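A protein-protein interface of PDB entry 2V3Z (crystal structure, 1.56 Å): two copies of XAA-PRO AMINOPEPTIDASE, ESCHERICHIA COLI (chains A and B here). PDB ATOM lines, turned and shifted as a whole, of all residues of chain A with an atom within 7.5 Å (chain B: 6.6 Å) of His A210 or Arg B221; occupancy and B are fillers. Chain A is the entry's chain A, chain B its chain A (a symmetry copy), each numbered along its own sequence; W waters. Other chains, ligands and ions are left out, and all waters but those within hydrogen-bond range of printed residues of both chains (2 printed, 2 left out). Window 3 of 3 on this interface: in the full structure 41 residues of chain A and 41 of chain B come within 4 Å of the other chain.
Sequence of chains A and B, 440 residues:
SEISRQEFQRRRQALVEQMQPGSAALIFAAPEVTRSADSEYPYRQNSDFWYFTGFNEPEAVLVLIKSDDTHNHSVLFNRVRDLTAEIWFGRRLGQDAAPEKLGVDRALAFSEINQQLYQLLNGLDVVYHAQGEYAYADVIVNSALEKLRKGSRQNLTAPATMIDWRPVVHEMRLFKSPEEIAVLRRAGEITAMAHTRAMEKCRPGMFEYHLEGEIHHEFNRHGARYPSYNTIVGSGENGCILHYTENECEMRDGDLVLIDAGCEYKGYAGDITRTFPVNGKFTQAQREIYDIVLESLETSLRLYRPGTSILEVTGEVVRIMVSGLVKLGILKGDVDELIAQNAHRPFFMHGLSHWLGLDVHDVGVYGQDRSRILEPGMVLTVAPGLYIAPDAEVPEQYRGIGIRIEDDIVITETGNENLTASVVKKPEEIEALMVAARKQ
Of the printed residues of chain B, His A210 touches Asn B220 (3.7 Å) and Arg B221 (3.1 Å). Printed residues of chain B within 4 Å of Gly A213: His B217 and Asn B220. Of the printed residues of chain B, Glu A214 touches His B217. Of the printed residues of chain A, Arg B221 touches His A210 (3.1 Å). Printed residues of chain A within 4 Å of Gly B223: Tyr A209. The nearest printed residue of chain A that does not touch Arg B221 is Tyr A209 (4.7 Å). The nearest printed residue of chain B that does not touch Gly A213 is His B216 (6.0 Å).
ND1 of His B217 is in hydrogen-bond range of NH1 of Arg B197 (2.9 Å). The side-chain carboxylate (OE1) of Glu A214 is in salt-bridge range of the guanidinium group (NE) of Arg A197, 2.8 Å away. The backbone NH (N) of Tyr A209 lies within hydrogen-bond range of the backbone carbonyl oxygen (O) of Asn A247. The side-chain amino group (NZ) of Lys A201 lies within salt-bridge range of the side-chain carboxylate (OE1) of Glu A214, 2.9 Å away. OE1 of Glu B218 lies within salt-bridge range of NE of Arg B221. N of Phe A207 is in hydrogen-bond range of ND1 of His A210 (3.1 Å).
Water W1 lies within hydrogen-bond range of the side-chain hydroxyl (OH) of Tyr A209 (2.8 Å), the backbone carbonyl oxygen (O) of Arg B221 (2.9 Å) and a ring nitrogen (NE2) of His A210 (3.4 Å). Water W2 bridges ND2 of Asn B220 and OE2 of Glu A212.
2 positions are printed for both chains.
Hydrophobic or aromatic side chains of chain B that line the printed part of chain A: His B217. Along chain B the printed residues that touch a printed residue of chain A span positions 217 to 223. Among the printed residues, no Asp or Glu carboxylate lies within 4 Å of a Lys or Arg side-chain nitrogen of the other chain.
CA of Gly B223 touches OH of Tyr A209, at 3.6 Å. CA of His A210 touches OD1 of Asn B220, 3.7 Å away. CD2 of His B217 touches O of Gly A213, 3.4 Å away. Gly A213 touches Asn B220 (N to ND2, 3.6 Å).
A ring nitrogen (NE2) of His A210 lies within hydrogen-bond range of the backbone carbonyl oxygen (O) of Arg B221 (3.1 Å). NE2 of His B217 lies within hydrogen-bond range of OE2 of Glu A214, at 2.9 Å. O of Tyr A209 is in hydrogen-bond range of ND2 of Asn B220 (2.9 Å).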
ATOM      1  N   ARG A 197      17.171   5.123  -0.781  1.00  0.00           N
ATOM      2  CA  ARG A 197      17.566   6.358  -0.112  1.00  0.00           C
ATOM      3  C   ARG A 197      16.475   7.415  -0.236  1.00  0.00           C
ATOM      4  O   ARG A 197      16.152   8.114   0.749  1.00  0.00           O
ATOM      5  CB  ARG A 197      18.867   6.860  -0.717  1.00  0.00           C
ATOM      6  CG  ARG A 197      19.353   8.180  -0.154  1.00  0.00           C
ATOM      7  CD  ARG A 197      20.672   8.553  -0.747  1.00  0.00           C
ATOM      8  NE  ARG A 197      21.092   9.895  -0.372  1.00  0.00           N
ATOM      9  CZ  ARG A 197      22.302  10.393  -0.621  1.00  0.00           C
ATOM     10  NH1 ARG A 197      23.238   9.634  -1.151  1.00  0.00           N
ATOM     11  NH2 ARG A 197      22.584  11.651  -0.320  1.00  0.00           N
ATOM     12  N   ALA A 198      15.908   7.570  -1.431  1.00  0.00           N
ATOM     13  CA  ALA A 198      14.842   8.545  -1.640  1.00  0.00           C
ATOM     14  C   ALA A 198      13.656   8.252  -0.727  1.00  0.00           C
ATOM     15  O   ALA A 198      13.102   9.174  -0.137  1.00  0.00           O
ATOM     16  CB  ALA A 198      14.404   8.557  -3.097  1.00  0.00           C
ATOM     17  N   LYS A 201      14.526   9.279   2.830  1.00  0.00           N
ATOM     18  CA  LYS A 201      14.739  10.703   3.018  1.00  0.00           C
ATOM     19  C   LYS A 201      13.473  11.532   2.889  1.00  0.00           C
ATOM     20  O   LYS A 201      13.387  12.595   3.468  1.00  0.00           O
ATOM     21  CB  LYS A 201      15.762  11.189   2.003  1.00  0.00           C
ATOM     22  CG  LYS A 201      17.152  10.608   2.241  1.00  0.00           C
ATOM     23  CD  LYS A 201      17.826  11.167   3.476  1.00  0.00           C
ATOM     24  CE  LYS A 201      19.156  10.469   3.737  1.00  0.00           C
ATOM     25  NZ  LYS A 201      20.234  10.988   2.892  1.00  0.00           N
ATOM     26  N   ARG A 203      10.200  13.484   3.125  1.00  0.00           N
ATOM     27  CA  ARG A 203       9.314  14.017   4.169  1.00  0.00           C
ATOM     28  C   ARG A 203       8.412  15.074   3.557  1.00  0.00           C
ATOM     29  O   ARG A 203       8.834  15.775   2.622  1.00  0.00           O
ATOM     30  CB  ARG A 203      10.091  14.658   5.308  1.00  0.00           C
ATOM     31  CG  ARG A 203      11.063  13.770   6.011  1.00  0.00           C
ATOM     32  CD  ARG A 203      10.414  12.707   6.908  1.00  0.00           C
ATOM     33  NE  ARG A 203      11.440  12.052   7.722  1.00  0.00           N
ATOM     34  CZ  ARG A 203      12.286  11.147   7.248  1.00  0.00           C
ATOM     35  NH1 ARG A 203      12.183  10.727   6.002  1.00  0.00           N
ATOM     36  NH2 ARG A 203      13.219  10.620   8.024  1.00  0.00           N
ATOM     37  N   GLY A 205       6.933  18.528   2.819  1.00  0.00           N
ATOM     38  CA  GLY A 205       7.621  19.818   2.851  1.00  0.00           C
ATOM     39  C   GLY A 205       8.886  19.914   2.042  1.00  0.00           C
ATOM     40  O   GLY A 205       9.299  21.019   1.667  1.00  0.00           O
ATOM     41  N   MET A 206       9.524  18.775   1.807  1.00  0.00           N
ATOM     42  CA  MET A 206      10.636  18.734   0.866  1.00  0.00           C
ATOM     43  C   MET A 206      10.098  18.982  -0.522  1.00  0.00           C
ATOM     44  O   MET A 206       8.942  18.702  -0.829  1.00  0.00           O
ATOM     45  CB  MET A 206      11.359  17.396   0.934  1.00  0.00           C
ATOM     46  CG  MET A 206      12.152  17.271   2.229  1.00  0.00           C
ATOM     47  SD  MET A 206      12.834  15.625   2.472  1.00  0.00           S
ATOM     48  CE  MET A 206      13.158  15.209   0.769  1.00  0.00           C
ATOM     49  N   PHE A 207      10.945  19.506  -1.382  1.00  0.00           N
ATOM     50  CA  PHE A 207      10.581  19.668  -2.765  1.00  0.00           C
ATOM     51  C   PHE A 207      10.929  18.417  -3.563  1.00  0.00           C
ATOM     52  O   PHE A 207      11.817  17.636  -3.214  1.00  0.00           O
ATOM     53  CB  PHE A 207      11.294  20.907  -3.339  1.00  0.00           C
ATOM     54  CG  PHE A 207      10.683  22.190  -2.890  1.00  0.00           C
ATOM     55  CD1 PHE A 207      10.918  22.670  -1.613  1.00  0.00           C
ATOM     56  CD2 PHE A 207       9.813  22.877  -3.717  1.00  0.00           C
ATOM     57  CE1 PHE A 207      10.308  23.843  -1.183  1.00  0.00           C
ATOM     58  CE2 PHE A 207       9.214  24.048  -3.295  1.00  0.00           C
ATOM     59  CZ  PHE A 207       9.456  24.519  -2.029  1.00  0.00           C
ATOM     60  N   GLU A 208      10.204  18.209  -4.662  1.00  0.00           N
ATOM     61  CA  GLU A 208      10.448  17.104  -5.556  1.00  0.00           C
ATOM     62  C   GLU A 208      11.931  17.029  -5.934  1.00  0.00           C
ATOM     63  O   GLU A 208      12.528  15.958  -5.920  1.00  0.00           O
ATOM     64  CB  GLU A 208       9.555  17.219  -6.792  1.00  0.00           C
ATOM     65  CG  GLU A 208       8.073  16.985  -6.507  1.00  0.00           C
ATOM     66  CD  GLU A 208       7.143  17.461  -7.615  1.00  0.00           C
ATOM     67  OE1 GLU A 208       7.520  18.365  -8.383  1.00  0.00           O
ATOM     68  OE2 GLU A 208       5.985  16.972  -7.653  1.00  0.00           O
ATOM     69  N   TYR A 209      12.533  18.183  -6.217  1.00  0.00           N
ATOM     70  CA  TYR A 209      13.929  18.202  -6.649  1.00  0.00           C
ATOM     71  C   TYR A 209      14.878  17.730  -5.552  1.00  0.00           C
ATOM     72  O   TYR A 209      15.966  17.239  -5.858  1.00  0.00           O
ATOM     73  CB  TYR A 209      14.377  19.554  -7.207  1.00  0.00           C
ATOM     74  CG  TYR A 209      14.318  20.710  -6.281  1.00  0.00           C
ATOM     75  CD1 TYR A 209      15.311  20.926  -5.331  1.00  0.00           C
ATOM     76  CD2 TYR A 209      13.292  21.653  -6.369  1.00  0.00           C
ATOM     77  CE1 TYR A 209      15.281  22.007  -4.489  1.00  0.00           C
ATOM     78  CE2 TYR A 209      13.246  22.720  -5.509  1.00  0.00           C
ATOM     79  CZ  TYR A 209      14.247  22.935  -4.586  1.00  0.00           C
ATOM     80  OH  TYR A 209      14.196  24.026  -3.727  1.00  0.00           O
ATOM     81  N   HIS A 210      14.476  17.810  -4.282  1.00  0.00           N
ATOM     82  CA  HIS A 210      15.342  17.308  -3.234  1.00  0.00           C
ATOM     83  C   HIS A 210      15.560  15.822  -3.347  1.00  0.00           C
ATOM     84  O   HIS A 210      16.660  15.309  -3.048  1.00  0.00           O
ATOM     85  CB  HIS A 210      14.793  17.634  -1.854  1.00  0.00           C
ATOM     86  CG  HIS A 210      14.968  19.055  -1.470  1.00  0.00           C
ATOM     87  ND1 HIS A 210      13.956  19.822  -0.937  1.00  0.00           N
ATOM     88  CD2 HIS A 210      16.041  19.874  -1.571  1.00  0.00           C
ATOM     89  CE1 HIS A 210      14.410  21.032  -0.680  1.00  0.00           C
ATOM     90  NE2 HIS A 210      15.675  21.093  -1.045  1.00  0.00           N
ATOM     91  N   LEU A 211      14.534  15.084  -3.770  1.00  0.00           N
ATOM     92  CA  LEU A 211      14.718  13.646  -3.943  1.00  0.00           C
ATOM     93  C   LEU A 211      15.618  13.327  -5.136  1.00  0.00           C
ATOM     94  O   LEU A 211      16.407  12.403  -5.104  1.00  0.00           O
ATOM     95  CB  LEU A 211      13.374  12.924  -4.031  1.00  0.00           C
ATOM     96  CG  LEU A 211      12.466  13.077  -2.810  1.00  0.00           C
ATOM     97  CD1 LEU A 211      11.233  12.173  -2.997  1.00  0.00           C
ATOM     98  CD2 LEU A 211      13.201  12.730  -1.542  1.00  0.00           C
ATOM     99  N   GLU A 212      15.495  14.130  -6.195  1.00  0.00           N
ATOM    100  CA  GLU A 212      16.437  14.064  -7.313  1.00  0.00           C
ATOM    101  C   GLU A 212      17.876  14.236  -6.791  1.00  0.00           C
ATOM    102  O   GLU A 212      18.782  13.504  -7.169  1.00  0.00           O
ATOM    103  CB  GLU A 212      16.080  15.133  -8.361  1.00  0.00           C
ATOM    104  CG  GLU A 212      17.138  15.362  -9.406  1.00  0.00           C
ATOM    105  CD  GLU A 212      16.759  16.484 -10.341  1.00  0.00           C
ATOM    106  OE1 GLU A 212      15.566  16.620 -10.606  1.00  0.00           O
ATOM    107  OE2 GLU A 212      17.642  17.263 -10.788  1.00  0.00           O
ATOM    108  N   GLY A 213      18.082  15.178  -5.879  1.00  0.00           N
ATOM    109  CA  GLY A 213      19.433  15.403  -5.353  1.00  0.00           C
ATOM    110  C   GLY A 213      19.969  14.211  -4.588  1.00  0.00           C
ATOM    111  O   GLY A 213      21.134  13.825  -4.737  1.00  0.00           O
ATOM    112  N   GLU A 214      19.120  13.610  -3.767  1.00  0.00           N
ATOM    113  CA  GLU A 214      19.516  12.408  -3.031  1.00  0.00           C
ATOM    114  C   GLU A 214      19.902  11.286  -3.989  1.00  0.00           C
ATOM    115  O   GLU A 214      20.891  10.585  -3.803  1.00  0.00           O
ATOM    116  CB  GLU A 214      18.376  11.937  -2.115  1.00  0.00           C
ATOM    117  CG  GLU A 214      17.995  12.910  -1.033  1.00  0.00           C
ATOM    118  CD  GLU A 214      19.099  13.193  -0.056  1.00  0.00           C
ATOM    119  OE1 GLU A 214      19.753  12.235   0.359  1.00  0.00           O
ATOM    120  OE2 GLU A 214      19.274  14.366   0.369  1.00  0.00           O
ATOM    121  N   ILE A 215      19.055  11.072  -4.994  1.00  0.00           N
ATOM    122  CA  ILE A 215      19.259  10.030  -6.004  1.00  0.00           C
ATOM    123  C   ILE A 215      20.568  10.224  -6.753  1.00  0.00           C
ATOM    124  O   ILE A 215      21.375   9.283  -6.886  1.00  0.00           O
ATOM    125  CB  ILE A 215      18.048   9.979  -6.944  1.00  0.00           C
ATOM    126  CG1 ILE A 215      16.851   9.420  -6.188  1.00  0.00           C
ATOM    127  CG2 ILE A 215      18.341   9.135  -8.209  1.00  0.00           C
ATOM    128  CD1 ILE A 215      15.569   9.590  -6.855  1.00  0.00           C
ATOM    129  N   HIS A 216      20.794  11.436  -7.256  1.00  0.00           N
ATOM    130  CA  HIS A 216      22.012  11.685  -8.003  1.00  0.00           C
ATOM    131  C   HIS A 216      23.273  11.540  -7.172  1.00  0.00           C
ATOM    132  O   HIS A 216      24.297  11.079  -7.674  1.00  0.00           O
ATOM    133  CB  HIS A 216      21.940  13.046  -8.661  1.00  0.00           C
ATOM    134  CG  HIS A 216      20.907  13.137  -9.730  1.00  0.00           C
ATOM    135  ND1 HIS A 216      20.612  14.332 -10.352  1.00  0.00           N
ATOM    136  CD2 HIS A 216      20.058  12.222 -10.245  1.00  0.00           C
ATOM    137  CE1 HIS A 216      19.662  14.120 -11.256  1.00  0.00           C
ATOM    138  NE2 HIS A 216      19.297  12.856 -11.204  1.00  0.00           N
ATOM    139  N   VAL A 233      10.372  13.121 -10.695  1.00  0.00           N
ATOM    140  CA  VAL A 233       9.893  13.076  -9.324  1.00  0.00           C
ATOM    141  C   VAL A 233       8.531  13.782  -9.314  1.00  0.00           C
ATOM    142  O   VAL A 233       8.446  14.996  -9.134  1.00  0.00           O
ATOM    143  CB  VAL A 233      10.856  13.724  -8.317  1.00  0.00           C
ATOM    144  CG1 VAL A 233      10.307  13.564  -6.897  1.00  0.00           C
ATOM    145  CG2 VAL A 233      12.270  13.110  -8.416  1.00  0.00           C
ATOM    146  N   ASN A 247      10.020  18.850 -11.493  1.00  0.00           N
ATOM    147  CA  ASN A 247      10.439  18.513 -10.128  1.00  0.00           C
ATOM    148  C   ASN A 247      10.476  19.737  -9.216  1.00  0.00           C
ATOM    149  O   ASN A 247      11.360  19.878  -8.377  1.00  0.00           O
ATOM    150  CB  ASN A 247      11.778  17.762 -10.140  1.00  0.00           C
ATOM    151  CG  ASN A 247      11.723  16.481 -10.951  1.00  0.00           C
ATOM    152  OD1 ASN A 247      10.652  16.058 -11.394  1.00  0.00           O
ATOM    153  ND2 ASN A 247      12.891  15.865 -11.172  1.00  0.00           N
ATOM    154  N   CSO A 249       7.731  21.129  -7.313  1.00  0.00           N
ATOM    155  CA  CSO A 249       6.697  21.347  -6.295  1.00  0.00           C
ATOM    156  CB  CSO A 249       5.384  20.726  -6.721  1.00  0.00           C
ATOM    157  SG  CSO A 249       4.805  21.413  -8.257  1.00  0.00           S
ATOM    158  C   CSO A 249       7.072  20.852  -4.917  1.00  0.00           C
ATOM    159  O   CSO A 249       7.879  19.942  -4.750  1.00  0.00           O
ATOM    160  OD  CSO A 249       4.421  22.825  -7.854  1.00  0.00           O
ATOM    161  N   MET A 251       6.337  18.737  -1.850  1.00  0.00           N
ATOM    162  CA  MET A 251       5.615  17.485  -1.669  1.00  0.00           C
ATOM    163  C   MET A 251       4.712  17.556  -0.431  1.00  0.00           C
ATOM    164  O   MET A 251       5.153  17.925   0.650  1.00  0.00           O
ATOM    165  CB  MET A 251       6.596  16.335  -1.550  1.00  0.00           C
ATOM    166  CG  MET A 251       7.404  16.110  -2.834  1.00  0.00           C
ATOM    167  SD  MET A 251       8.535  14.722  -2.748  1.00  0.00           S
ATOM    168  CE  MET A 251       9.634  15.259  -1.417  1.00  0.00           C
ATOM    169  N   MET B 193      28.881  27.533  -0.011  1.00  0.00           N
ATOM    170  CA  MET B 193      28.486  26.430   0.900  1.00  0.00           C
ATOM    171  C   MET B 193      28.947  25.078   0.342  1.00  0.00           C
ATOM    172  O   MET B 193      29.373  24.167   1.077  1.00  0.00           O
ATOM    173  CB  MET B 193      26.991  26.419   1.178  1.00  0.00           C
ATOM    174  CG  MET B 193      26.575  27.478   2.103  1.00  0.00           C
ATOM    175  SD  MET B 193      24.847  27.398   2.636  1.00  0.00           S
ATOM    176  CE  MET B 193      23.991  28.054   1.231  1.00  0.00           C
ATOM    177  N   ARG B 197      31.646  22.459   1.989  1.00  0.00           N
ATOM    178  CA  ARG B 197      31.288  21.057   2.173  1.00  0.00           C
ATOM    179  C   ARG B 197      32.347  20.142   1.569  1.00  0.00           C
ATOM    180  O   ARG B 197      32.739  19.129   2.187  1.00  0.00           O
ATOM    181  CB  ARG B 197      29.933  20.799   1.535  1.00  0.00           C
ATOM    182  CG  ARG B 197      29.474  19.356   1.597  1.00  0.00           C
ATOM    183  CD  ARG B 197      28.104  19.212   1.020  1.00  0.00           C
ATOM    184  NE  ARG B 197      27.694  17.822   0.895  1.00  0.00           N
ATOM    185  CZ  ARG B 197      26.460  17.435   0.580  1.00  0.00           C
ATOM    186  NH1 ARG B 197      25.496  18.322   0.454  1.00  0.00           N
ATOM    187  NH2 ARG B 197      26.184  16.151   0.406  1.00  0.00           N
ATOM    188  N   HIS B 216      27.390  18.995  -6.061  1.00  0.00           N
ATOM    189  CA  HIS B 216      26.110  19.026  -6.742  1.00  0.00           C
ATOM    190  C   HIS B 216      24.925  18.827  -5.815  1.00  0.00           C
ATOM    191  O   HIS B 216      23.871  19.426  -6.018  1.00  0.00           O
ATOM    192  CB  HIS B 216      26.104  18.015  -7.867  1.00  0.00           C
ATOM    193  CG  HIS B 216      27.043  18.351  -8.975  1.00  0.00           C
ATOM    194  ND1 HIS B 216      27.264  17.484 -10.023  1.00  0.00           N
ATOM    195  CD2 HIS B 216      27.860  19.406  -9.176  1.00  0.00           C
ATOM    196  CE1 HIS B 216      28.138  18.036 -10.858  1.00  0.00           C
ATOM    197  NE2 HIS B 216      28.528  19.193 -10.363  1.00  0.00           N
ATOM    198  N   HIS B 217      25.093  17.989  -4.785  1.00  0.00           N
ATOM    199  CA  HIS B 217      24.035  17.778  -3.807  1.00  0.00           C
ATOM    200  C   HIS B 217      23.778  19.070  -3.045  1.00  0.00           C
ATOM    201  O   HIS B 217      22.615  19.444  -2.814  1.00  0.00           O
ATOM    202  CB  HIS B 217      24.402  16.646  -2.865  1.00  0.00           C
ATOM    203  CG  HIS B 217      23.336  16.318  -1.884  1.00  0.00           C
ATOM    204  ND1 HIS B 217      23.217  16.989  -0.683  1.00  0.00           N
ATOM    205  CD2 HIS B 217      22.309  15.436  -1.928  1.00  0.00           C
ATOM    206  CE1 HIS B 217      22.185  16.496  -0.013  1.00  0.00           C
ATOM    207  NE2 HIS B 217      21.626  15.542  -0.740  1.00  0.00           N
ATOM    208  N   GLU B 218      24.843  19.794  -2.689  1.00  0.00           N
ATOM    209  CA  GLU B 218      24.676  21.041  -1.943  1.00  0.00           C
ATOM    210  C   GLU B 218      23.989  22.106  -2.824  1.00  0.00           C
ATOM    211  O   GLU B 218      23.104  22.815  -2.374  1.00  0.00           O
ATOM    212  CB  GLU B 218      26.000  21.547  -1.426  1.00  0.00           C
ATOM    213  CG  GLU B 218      25.836  22.725  -0.459  1.00  0.00           C
ATOM    214  CD  GLU B 218      25.287  22.328   0.873  1.00  0.00           C
ATOM    215  OE1 GLU B 218      25.218  21.124   1.226  1.00  0.00           O
ATOM    216  OE2 GLU B 218      24.915  23.272   1.629  1.00  0.00           O
ATOM    217  N   PHE B 219      24.367  22.200  -4.096  1.00  0.00           N
ATOM    218  CA  PHE B 219      23.673  23.098  -5.019  1.00  0.00           C
ATOM    219  C   PHE B 219      22.177  22.803  -4.986  1.00  0.00           C
ATOM    220  O   PHE B 219      21.333  23.695  -4.826  1.00  0.00           O
ATOM    221  CB  PHE B 219      24.151  22.896  -6.463  1.00  0.00           C
ATOM    222  CG  PHE B 219      25.541  23.362  -6.782  1.00  0.00           C
ATOM    223  CD1 PHE B 219      26.344  24.088  -5.913  1.00  0.00           C
ATOM    224  CD2 PHE B 219      26.060  23.022  -8.041  1.00  0.00           C
ATOM    225  CE1 PHE B 219      27.635  24.492  -6.300  1.00  0.00           C
ATOM    226  CE2 PHE B 219      27.335  23.426  -8.418  1.00  0.00           C
ATOM    227  CZ  PHE B 219      28.116  24.146  -7.543  1.00  0.00           C
ATOM    228  N   ASN B 220      21.853  21.528  -5.166  1.00  0.00           N
ATOM    229  CA  ASN B 220      20.468  21.076  -5.247  1.00  0.00           C
ATOM    230  C   ASN B 220      19.662  21.409  -4.034  1.00  0.00           C
ATOM    231  O   ASN B 220      18.523  21.868  -4.149  1.00  0.00           O
ATOM    232  CB  ASN B 220      20.421  19.572  -5.550  1.00  0.00           C
ATOM    233  CG  ASN B 220      19.023  18.980  -5.429  1.00  0.00           C
ATOM    234  OD1 ASN B 220      18.517  18.773  -4.326  1.00  0.00           O
ATOM    235  ND2 ASN B 220      18.414  18.686  -6.565  1.00  0.00           N
ATOM    236  N   ARG B 221      20.245  21.237  -2.863  1.00  0.00           N
ATOM    237  CA  ARG B 221      19.424  21.386  -1.677  1.00  0.00           C
ATOM    238  C   ARG B 221      18.990  22.837  -1.444  1.00  0.00           C
ATOM    239  O   ARG B 221      17.990  23.084  -0.764  1.00  0.00           O
ATOM    240  CB  ARG B 221      20.065  20.719  -0.482  1.00  0.00           C
ATOM    241  CG  ARG B 221      21.216  21.387   0.089  1.00  0.00           C
ATOM    242  CD  ARG B 221      21.716  20.576   1.279  1.00  0.00           C
ATOM    243  NE  ARG B 221      22.540  21.404   2.133  1.00  0.00           N
ATOM    244  CZ  ARG B 221      22.091  22.167   3.125  1.00  0.00           C
ATOM    245  NH1 ARG B 221      20.809  22.178   3.473  1.00  0.00           N
ATOM    246  NH2 ARG B 221      22.960  22.904   3.803  1.00  0.00           N
ATOM    247  N   HIS B 222      19.714  23.785  -2.055  1.00  0.00           N
ATOM    248  CA  HIS B 222      19.352  25.214  -2.020  1.00  0.00           C
ATOM    249  C   HIS B 222      18.564  25.678  -3.235  1.00  0.00           C
ATOM    250  O   HIS B 222      18.296  26.862  -3.376  1.00  0.00           O
ATOM    251  CB  HIS B 222      20.587  26.081  -1.815  1.00  0.00           C
ATOM    252  CG  HIS B 222      21.348  25.726  -0.595  1.00  0.00           C
ATOM    253  ND1 HIS B 222      20.837  25.942   0.673  1.00  0.00           N
ATOM    254  CD2 HIS B 222      22.534  25.100  -0.426  1.00  0.00           C
ATOM    255  CE1 HIS B 222      21.705  25.497   1.563  1.00  0.00           C
ATOM    256  NE2 HIS B 222      22.743  24.978   0.923  1.00  0.00           N
ATOM    257  N   GLY B 223      18.165  24.749  -4.098  1.00  0.00           N
ATOM    258  CA  GLY B 223      17.332  25.071  -5.227  1.00  0.00           C
ATOM    259  C   GLY B 223      18.085  25.475  -6.460  1.00  0.00           C
ATOM    260  O   GLY B 223      17.476  26.070  -7.360  1.00  0.00           O
ATOM    261  N   ALA B 224      19.391  25.199  -6.519  1.00  0.00           N
ATOM    262  CA  ALA B 224      20.145  25.349  -7.760  1.00  0.00           C
ATOM    263  C   ALA B 224      20.347  23.955  -8.332  1.00  0.00           C
ATOM    264  O   ALA B 224      21.243  23.210  -7.952  1.00  0.00           O
ATOM    265  CB  ALA B 224      21.445  26.055  -7.534  1.00  0.00           C
HETATM  266  O   HOH W   1      15.524  24.450  -1.340  1.00  0.00           O
HETATM  267  O   HOH W   2      19.796  18.471  -9.126  1.00  0.00           O
